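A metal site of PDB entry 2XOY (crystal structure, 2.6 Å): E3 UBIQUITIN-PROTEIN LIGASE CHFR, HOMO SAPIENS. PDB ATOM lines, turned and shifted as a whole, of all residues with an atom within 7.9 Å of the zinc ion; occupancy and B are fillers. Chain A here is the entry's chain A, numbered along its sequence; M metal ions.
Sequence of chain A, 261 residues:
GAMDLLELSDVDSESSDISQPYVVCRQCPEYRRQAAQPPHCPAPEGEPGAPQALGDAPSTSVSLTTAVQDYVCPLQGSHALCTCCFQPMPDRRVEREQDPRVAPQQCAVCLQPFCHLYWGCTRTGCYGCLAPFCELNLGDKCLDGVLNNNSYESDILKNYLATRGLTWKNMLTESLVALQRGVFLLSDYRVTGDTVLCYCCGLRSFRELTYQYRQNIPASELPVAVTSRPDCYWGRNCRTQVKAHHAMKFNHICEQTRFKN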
ATOM      1  N   VAL A  23       6.375 -33.019  -7.896  1.00  0.00           N
ATOM      2  CA  VAL A  23       5.110 -32.369  -7.538  1.00  0.00           C
ATOM      3  C   VAL A  23       5.050 -30.856  -7.731  1.00  0.00           C
ATOM      4  O   VAL A  23       5.841 -30.105  -7.186  1.00  0.00           O
ATOM      5  CB  VAL A  23       4.754 -32.635  -6.070  1.00  0.00           C
ATOM      6  CG1 VAL A  23       3.659 -31.695  -5.631  1.00  0.00           C
ATOM      7  CG2 VAL A  23       4.336 -34.072  -5.886  1.00  0.00           C
ATOM      8  N   VAL A  24       4.051 -30.411  -8.490  1.00  0.00           N
ATOM      9  CA  VAL A  24       3.840 -28.988  -8.747  1.00  0.00           C
ATOM     10  C   VAL A  24       2.406 -28.594  -8.426  1.00  0.00           C
ATOM     11  O   VAL A  24       1.465 -29.078  -9.055  1.00  0.00           O
ATOM     12  CB  VAL A  24       4.094 -28.667 -10.236  1.00  0.00           C
ATOM     13  CG1 VAL A  24       3.440 -27.361 -10.639  1.00  0.00           C
ATOM     14  CG2 VAL A  24       5.605 -28.661 -10.514  1.00  0.00           C
ATOM     15  N   CYS A  25       2.232 -27.703  -7.442  1.00  0.00           N
ATOM     16  CA  CYS A  25       0.906 -27.310  -6.970  1.00  0.00           C
ATOM     17  C   CYS A  25       0.631 -25.820  -7.192  1.00  0.00           C
ATOM     18  O   CYS A  25       1.493 -25.097  -7.680  1.00  0.00           O
ATOM     19  CB  CYS A  25       0.740 -27.605  -5.485  1.00  0.00           C
ATOM     20  SG  CYS A  25       1.262 -26.240  -4.442  1.00  0.00           S
ATOM     21  N   ARG A  26      -0.578 -25.390  -6.817  1.00  0.00           N
ATOM     22  CA  ARG A  26      -1.004 -23.992  -6.942  1.00  0.00           C
ATOM     23  C   ARG A  26      -0.065 -22.971  -6.283  1.00  0.00           C
ATOM     24  O   ARG A  26       0.038 -21.834  -6.742  1.00  0.00           O
ATOM     25  CB  ARG A  26      -2.406 -23.805  -6.368  1.00  0.00           C
ATOM     26  CG  ARG A  26      -3.528 -24.306  -7.256  1.00  0.00           C
ATOM     27  CD  ARG A  26      -4.837 -23.736  -6.787  1.00  0.00           C
ATOM     28  NE  ARG A  26      -5.785 -24.759  -6.376  1.00  0.00           N
ATOM     29  CZ  ARG A  26      -6.817 -24.547  -5.561  1.00  0.00           C
ATOM     30  NH1 ARG A  26      -7.010 -23.330  -5.056  1.00  0.00           N
ATOM     31  NH2 ARG A  26      -7.637 -25.537  -5.234  1.00  0.00           N
ATOM     32  N   GLN A  27       0.602 -23.364  -5.209  1.00  0.00           N
ATOM     33  CA  GLN A  27       1.453 -22.444  -4.452  1.00  0.00           C
ATOM     34  C   GLN A  27       2.940 -22.737  -4.675  1.00  0.00           C
ATOM     35  O   GLN A  27       3.796 -22.205  -3.963  1.00  0.00           O
ATOM     36  CB  GLN A  27       1.125 -22.521  -2.961  1.00  0.00           C
ATOM     37  CG  GLN A  27      -0.201 -21.888  -2.547  1.00  0.00           C
ATOM     38  CD  GLN A  27      -0.449 -21.965  -1.044  1.00  0.00           C
ATOM     39  OE1 GLN A  27       0.142 -22.778  -0.338  1.00  0.00           O
ATOM     40  NE2 GLN A  27      -1.333 -21.105  -0.548  1.00  0.00           N
ATOM     41  N   CYS A  28       3.233 -23.576  -5.662  1.00  0.00           N
ATOM     42  CA  CYS A  28       4.614 -23.891  -6.029  1.00  0.00           C
ATOM     43  C   CYS A  28       5.254 -22.709  -6.752  1.00  0.00           C
ATOM     44  O   CYS A  28       4.621 -22.064  -7.587  1.00  0.00           O
ATOM     45  CB  CYS A  28       4.703 -25.150  -6.896  1.00  0.00           C
ATOM     46  SG  CYS A  28       4.866 -26.739  -6.001  1.00  0.00           S
ATOM     47  N   PRO A  29       6.525 -22.413  -6.438  1.00  0.00           N
ATOM     48  CA  PRO A  29       7.269 -21.312  -7.081  1.00  0.00           C
ATOM     49  C   PRO A  29       7.465 -21.573  -8.581  1.00  0.00           C
ATOM     50  O   PRO A  29       7.467 -22.724  -9.018  1.00  0.00           O
ATOM     51  CB  PRO A  29       8.626 -21.330  -6.359  1.00  0.00           C
ATOM     52  CG  PRO A  29       8.745 -22.713  -5.773  1.00  0.00           C
ATOM     53  CD  PRO A  29       7.349 -23.152  -5.455  1.00  0.00           C
ATOM     54  N   ARG A  32       9.896 -24.306 -10.133  1.00  0.00           N
ATOM     55  CA  ARG A  32       9.442 -25.682 -10.034  1.00  0.00           C
ATOM     56  C   ARG A  32       8.582 -26.001 -11.243  1.00  0.00           C
ATOM     57  O   ARG A  32       8.661 -27.087 -11.811  1.00  0.00           O
ATOM     58  CB  ARG A  32       8.632 -25.911  -8.754  1.00  0.00           C
ATOM     59  CG  ARG A  32       9.445 -26.110  -7.472  1.00  0.00           C
ATOM     60  CD  ARG A  32       9.766 -27.585  -7.217  1.00  0.00           C
ATOM     61  NE  ARG A  32       8.725 -28.290  -6.460  1.00  0.00           N
ATOM     62  CZ  ARG A  32       8.694 -29.609  -6.298  1.00  0.00           C
ATOM     63  NH1 ARG A  32       9.644 -30.376  -6.822  1.00  0.00           N
ATOM     64  NH2 ARG A  32       7.711 -30.175  -5.596  1.00  0.00           N
ATOM     65  N   TYR A  71       1.467 -18.358   0.610  1.00  0.00           N
ATOM     66  CA  TYR A  71       2.529 -19.348   0.806  1.00  0.00           C
ATOM     67  C   TYR A  71       3.310 -19.629  -0.498  1.00  0.00           C
ATOM     68  O   TYR A  71       2.878 -19.270  -1.592  1.00  0.00           O
ATOM     69  CB  TYR A  71       1.915 -20.640   1.342  1.00  0.00           C
ATOM     70  CG  TYR A  71       2.867 -21.608   2.023  1.00  0.00           C
ATOM     71  CD1 TYR A  71       3.135 -22.846   1.445  1.00  0.00           C
ATOM     72  CD2 TYR A  71       3.469 -21.300   3.235  1.00  0.00           C
ATOM     73  CE1 TYR A  71       3.990 -23.749   2.060  1.00  0.00           C
ATOM     74  CE2 TYR A  71       4.328 -22.197   3.856  1.00  0.00           C
ATOM     75  CZ  TYR A  71       4.575 -23.428   3.268  1.00  0.00           C
ATOM     76  OH  TYR A  71       5.419 -24.344   3.856  1.00  0.00           O
ATOM     77  N   VAL A  72       4.470 -20.257  -0.344  1.00  0.00           N
ATOM     78  CA  VAL A  72       5.247 -20.742  -1.467  1.00  0.00           C
ATOM     79  C   VAL A  72       6.078 -21.906  -0.978  1.00  0.00           C
ATOM     80  O   VAL A  72       6.873 -21.760  -0.052  1.00  0.00           O
ATOM     81  CB  VAL A  72       6.196 -19.670  -2.023  1.00  0.00           C
ATOM     82  CG1 VAL A  72       7.281 -20.332  -2.849  1.00  0.00           C
ATOM     83  CG2 VAL A  72       5.412 -18.675  -2.854  1.00  0.00           C
ATOM     84  N   CYS A  73       5.889 -23.056  -1.591  1.00  0.00           N
ATOM     85  CA  CYS A  73       6.533 -24.268  -1.106  1.00  0.00           C
ATOM     86  C   CYS A  73       8.054 -24.177  -1.242  1.00  0.00           C
ATOM     87  O   CYS A  73       8.578 -23.800  -2.289  1.00  0.00           O
ATOM     88  CB  CYS A  73       5.990 -25.493  -1.841  1.00  0.00           C
ATOM     89  SG  CYS A  73       4.184 -25.511  -1.943  1.00  0.00           S
ATOM     90  N   PRO A  74       8.753 -24.506  -0.146  1.00  0.00           N
ATOM     91  CA  PRO A  74      10.230 -24.525  -0.063  1.00  0.00           C
ATOM     92  C   PRO A  74      10.845 -25.797  -0.655  1.00  0.00           C
ATOM     93  O   PRO A  74      10.127 -26.710  -1.050  1.00  0.00           O
ATOM     94  CB  PRO A  74      10.487 -24.482   1.451  1.00  0.00           C
ATOM     95  CG  PRO A  74       9.269 -25.107   2.050  1.00  0.00           C
ATOM     96  CD  PRO A  74       8.120 -24.743   1.155  1.00  0.00           C
ATOM     97  N   GLY A  77       9.877 -28.432   1.353  1.00  0.00           N
ATOM     98  CA  GLY A  77       8.432 -28.409   1.465  1.00  0.00           C
ATOM     99  C   GLY A  77       7.839 -29.684   0.907  1.00  0.00           C
ATOM    100  O   GLY A  77       8.178 -30.115  -0.197  1.00  0.00           O
ATOM    101  N   SER A  78       6.964 -30.300   1.701  1.00  0.00           N
ATOM    102  CA  SER A  78       6.238 -31.481   1.272  1.00  0.00           C
ATOM    103  C   SER A  78       4.898 -31.068   0.685  1.00  0.00           C
ATOM    104  O   SER A  78       4.473 -29.902   0.812  1.00  0.00           O
ATOM    105  CB  SER A  78       6.010 -32.432   2.451  1.00  0.00           C
ATOM    106  OG  SER A  78       7.243 -32.867   2.988  1.00  0.00           O
ATOM    107  N   HIS A  79       4.236 -32.009   0.033  1.00  0.00           N
ATOM    108  CA  HIS A  79       2.871 -31.798  -0.427  1.00  0.00           C
ATOM    109  C   HIS A  79       2.033 -32.976   0.027  1.00  0.00           C
ATOM    110  O   HIS A  79       2.536 -34.101   0.136  1.00  0.00           O
ATOM    111  CB  HIS A  79       2.818 -31.640  -1.946  1.00  0.00           C
ATOM    112  CG  HIS A  79       3.503 -30.405  -2.455  1.00  0.00           C
ATOM    113  ND1 HIS A  79       4.870 -30.294  -2.529  1.00  0.00           N
ATOM    114  CD2 HIS A  79       2.996 -29.240  -2.931  1.00  0.00           C
ATOM    115  CE1 HIS A  79       5.189 -29.101  -3.011  1.00  0.00           C
ATOM    116  NE2 HIS A  79       4.073 -28.446  -3.269  1.00  0.00           N
ATOM    117  N   PRO A  88      -2.578 -31.846  -5.130  1.00  0.00           N
ATOM    118  CA  PRO A  88      -1.544 -31.567  -4.116  1.00  0.00           C
ATOM    119  C   PRO A  88      -1.638 -30.193  -3.458  1.00  0.00           C
ATOM    120  O   PRO A  88      -1.897 -29.188  -4.117  1.00  0.00           O
ATOM    121  CB  PRO A  88      -0.256 -31.621  -4.926  1.00  0.00           C
ATOM    122  CG  PRO A  88      -0.676 -31.204  -6.289  1.00  0.00           C
ATOM    123  CD  PRO A  88      -2.016 -31.830  -6.489  1.00  0.00           C
ATOM    124  N   MET A  89      -1.422 -30.173  -2.145  1.00  0.00           N
ATOM    125  CA  MET A  89      -1.265 -28.937  -1.381  1.00  0.00           C
ATOM    126  C   MET A  89      -0.016 -29.093  -0.528  1.00  0.00           C
ATOM    127  O   MET A  89       0.423 -30.216  -0.254  1.00  0.00           O
ATOM    128  CB  MET A  89      -2.469 -28.702  -0.480  1.00  0.00           C
ATOM    129  CG  MET A  89      -2.647 -29.784   0.566  1.00  0.00           C
ATOM    130  SD  MET A  89      -4.234 -29.676   1.416  1.00  0.00           S
ATOM    131  CE  MET A  89      -4.174 -31.152   2.433  1.00  0.00           C
ATOM    132  N   PRO A  90       0.575 -27.973  -0.093  1.00  0.00           N
ATOM    133  CA  PRO A  90       1.744 -28.071   0.784  1.00  0.00           C
ATOM    134  C   PRO A  90       1.333 -28.709   2.103  1.00  0.00           C
ATOM    135  O   PRO A  90       0.316 -28.297   2.640  1.00  0.00           O
ATOM    136  CB  PRO A  90       2.108 -26.602   1.022  1.00  0.00           C
ATOM    137  CG  PRO A  90       0.866 -25.828   0.660  1.00  0.00           C
ATOM    138  CD  PRO A  90       0.264 -26.579  -0.458  1.00  0.00           C
ATOM    139  N   ASP A  91       2.087 -29.689   2.594  1.00  0.00           N
ATOM    140  CA  ASP A  91       1.732 -30.306   3.872  1.00  0.00           C
ATOM    141  C   ASP A  91       2.249 -29.471   5.052  1.00  0.00           C
ATOM    142  O   ASP A  91       3.437 -29.508   5.369  1.00  0.00           O
ATOM    143  CB  ASP A  91       2.244 -31.748   3.972  1.00  0.00           C
ATOM    144  CG  ASP A  91       1.804 -32.438   5.254  1.00  0.00           C
ATOM    145  OD1 ASP A  91       1.551 -33.668   5.231  1.00  0.00           O
ATOM    146  OD2 ASP A  91       1.677 -31.754   6.293  1.00  0.00           O
ATOM    147  N   TRP A 119      -7.403 -23.693   0.867  1.00  0.00           N
ATOM    148  CA  TRP A 119      -7.481 -22.794  -0.299  1.00  0.00           C
ATOM    149  C   TRP A 119      -8.666 -23.022  -1.238  1.00  0.00           C
ATOM    150  O   TRP A 119      -8.641 -22.551  -2.376  1.00  0.00           O
ATOM    151  CB  TRP A 119      -6.179 -22.838  -1.111  1.00  0.00           C
ATOM    152  CG  TRP A 119      -5.856 -24.193  -1.716  1.00  0.00           C
ATOM    153  CD1 TRP A 119      -6.700 -25.249  -1.853  1.00  0.00           C
ATOM    154  CD2 TRP A 119      -4.597 -24.604  -2.267  1.00  0.00           C
ATOM    155  NE1 TRP A 119      -6.039 -26.303  -2.448  1.00  0.00           N
ATOM    156  CE2 TRP A 119      -4.751 -25.938  -2.715  1.00  0.00           C
ATOM    157  CE3 TRP A 119      -3.350 -23.987  -2.439  1.00  0.00           C
ATOM    158  CZ2 TRP A 119      -3.706 -26.656  -3.302  1.00  0.00           C
ATOM    159  CZ3 TRP A 119      -2.322 -24.698  -3.022  1.00  0.00           C
ATOM    160  CH2 TRP A 119      -2.500 -26.021  -3.450  1.00  0.00           C
HETATM  161 ZN    ZN M   1       3.524 -26.550  -3.981  1.00  0.00          ZN
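The side-chain sulfur (SG) of Cys 25 lies close to the backbone NH (N) of Gln 27, at 3.0 Å.
The backbone NH of Cys 73 is in hydrogen-bond range of the backbone carbonyl oxygen of Gln 27.
The backbone carbonyl oxygen (O) of Val 23 lies close to the side-chain sulfur (SG) of Cys 28 (3.7 Å).
Gln 27 touches the zinc ion (C to ZN, 3.9 Å).
Within 4 Å of the zinc ion: Cys 25, Gln 27, Cys 28, Cys 73 and His 79.
The nearest printed residue that does not touch the zinc ion is Pro 90 (4.8 Å).
NE2 of His 79 binds the zinc ion, at 2.1 Å.
SG of Cys 25 is bound to the zinc ion (2.3 Å).
The zinc ion is bound by the side-chain sulfur (SG) of Cys 73 (2.4 Å).
SG of Cys 28 is bound to the zinc ion (2.4 Å).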
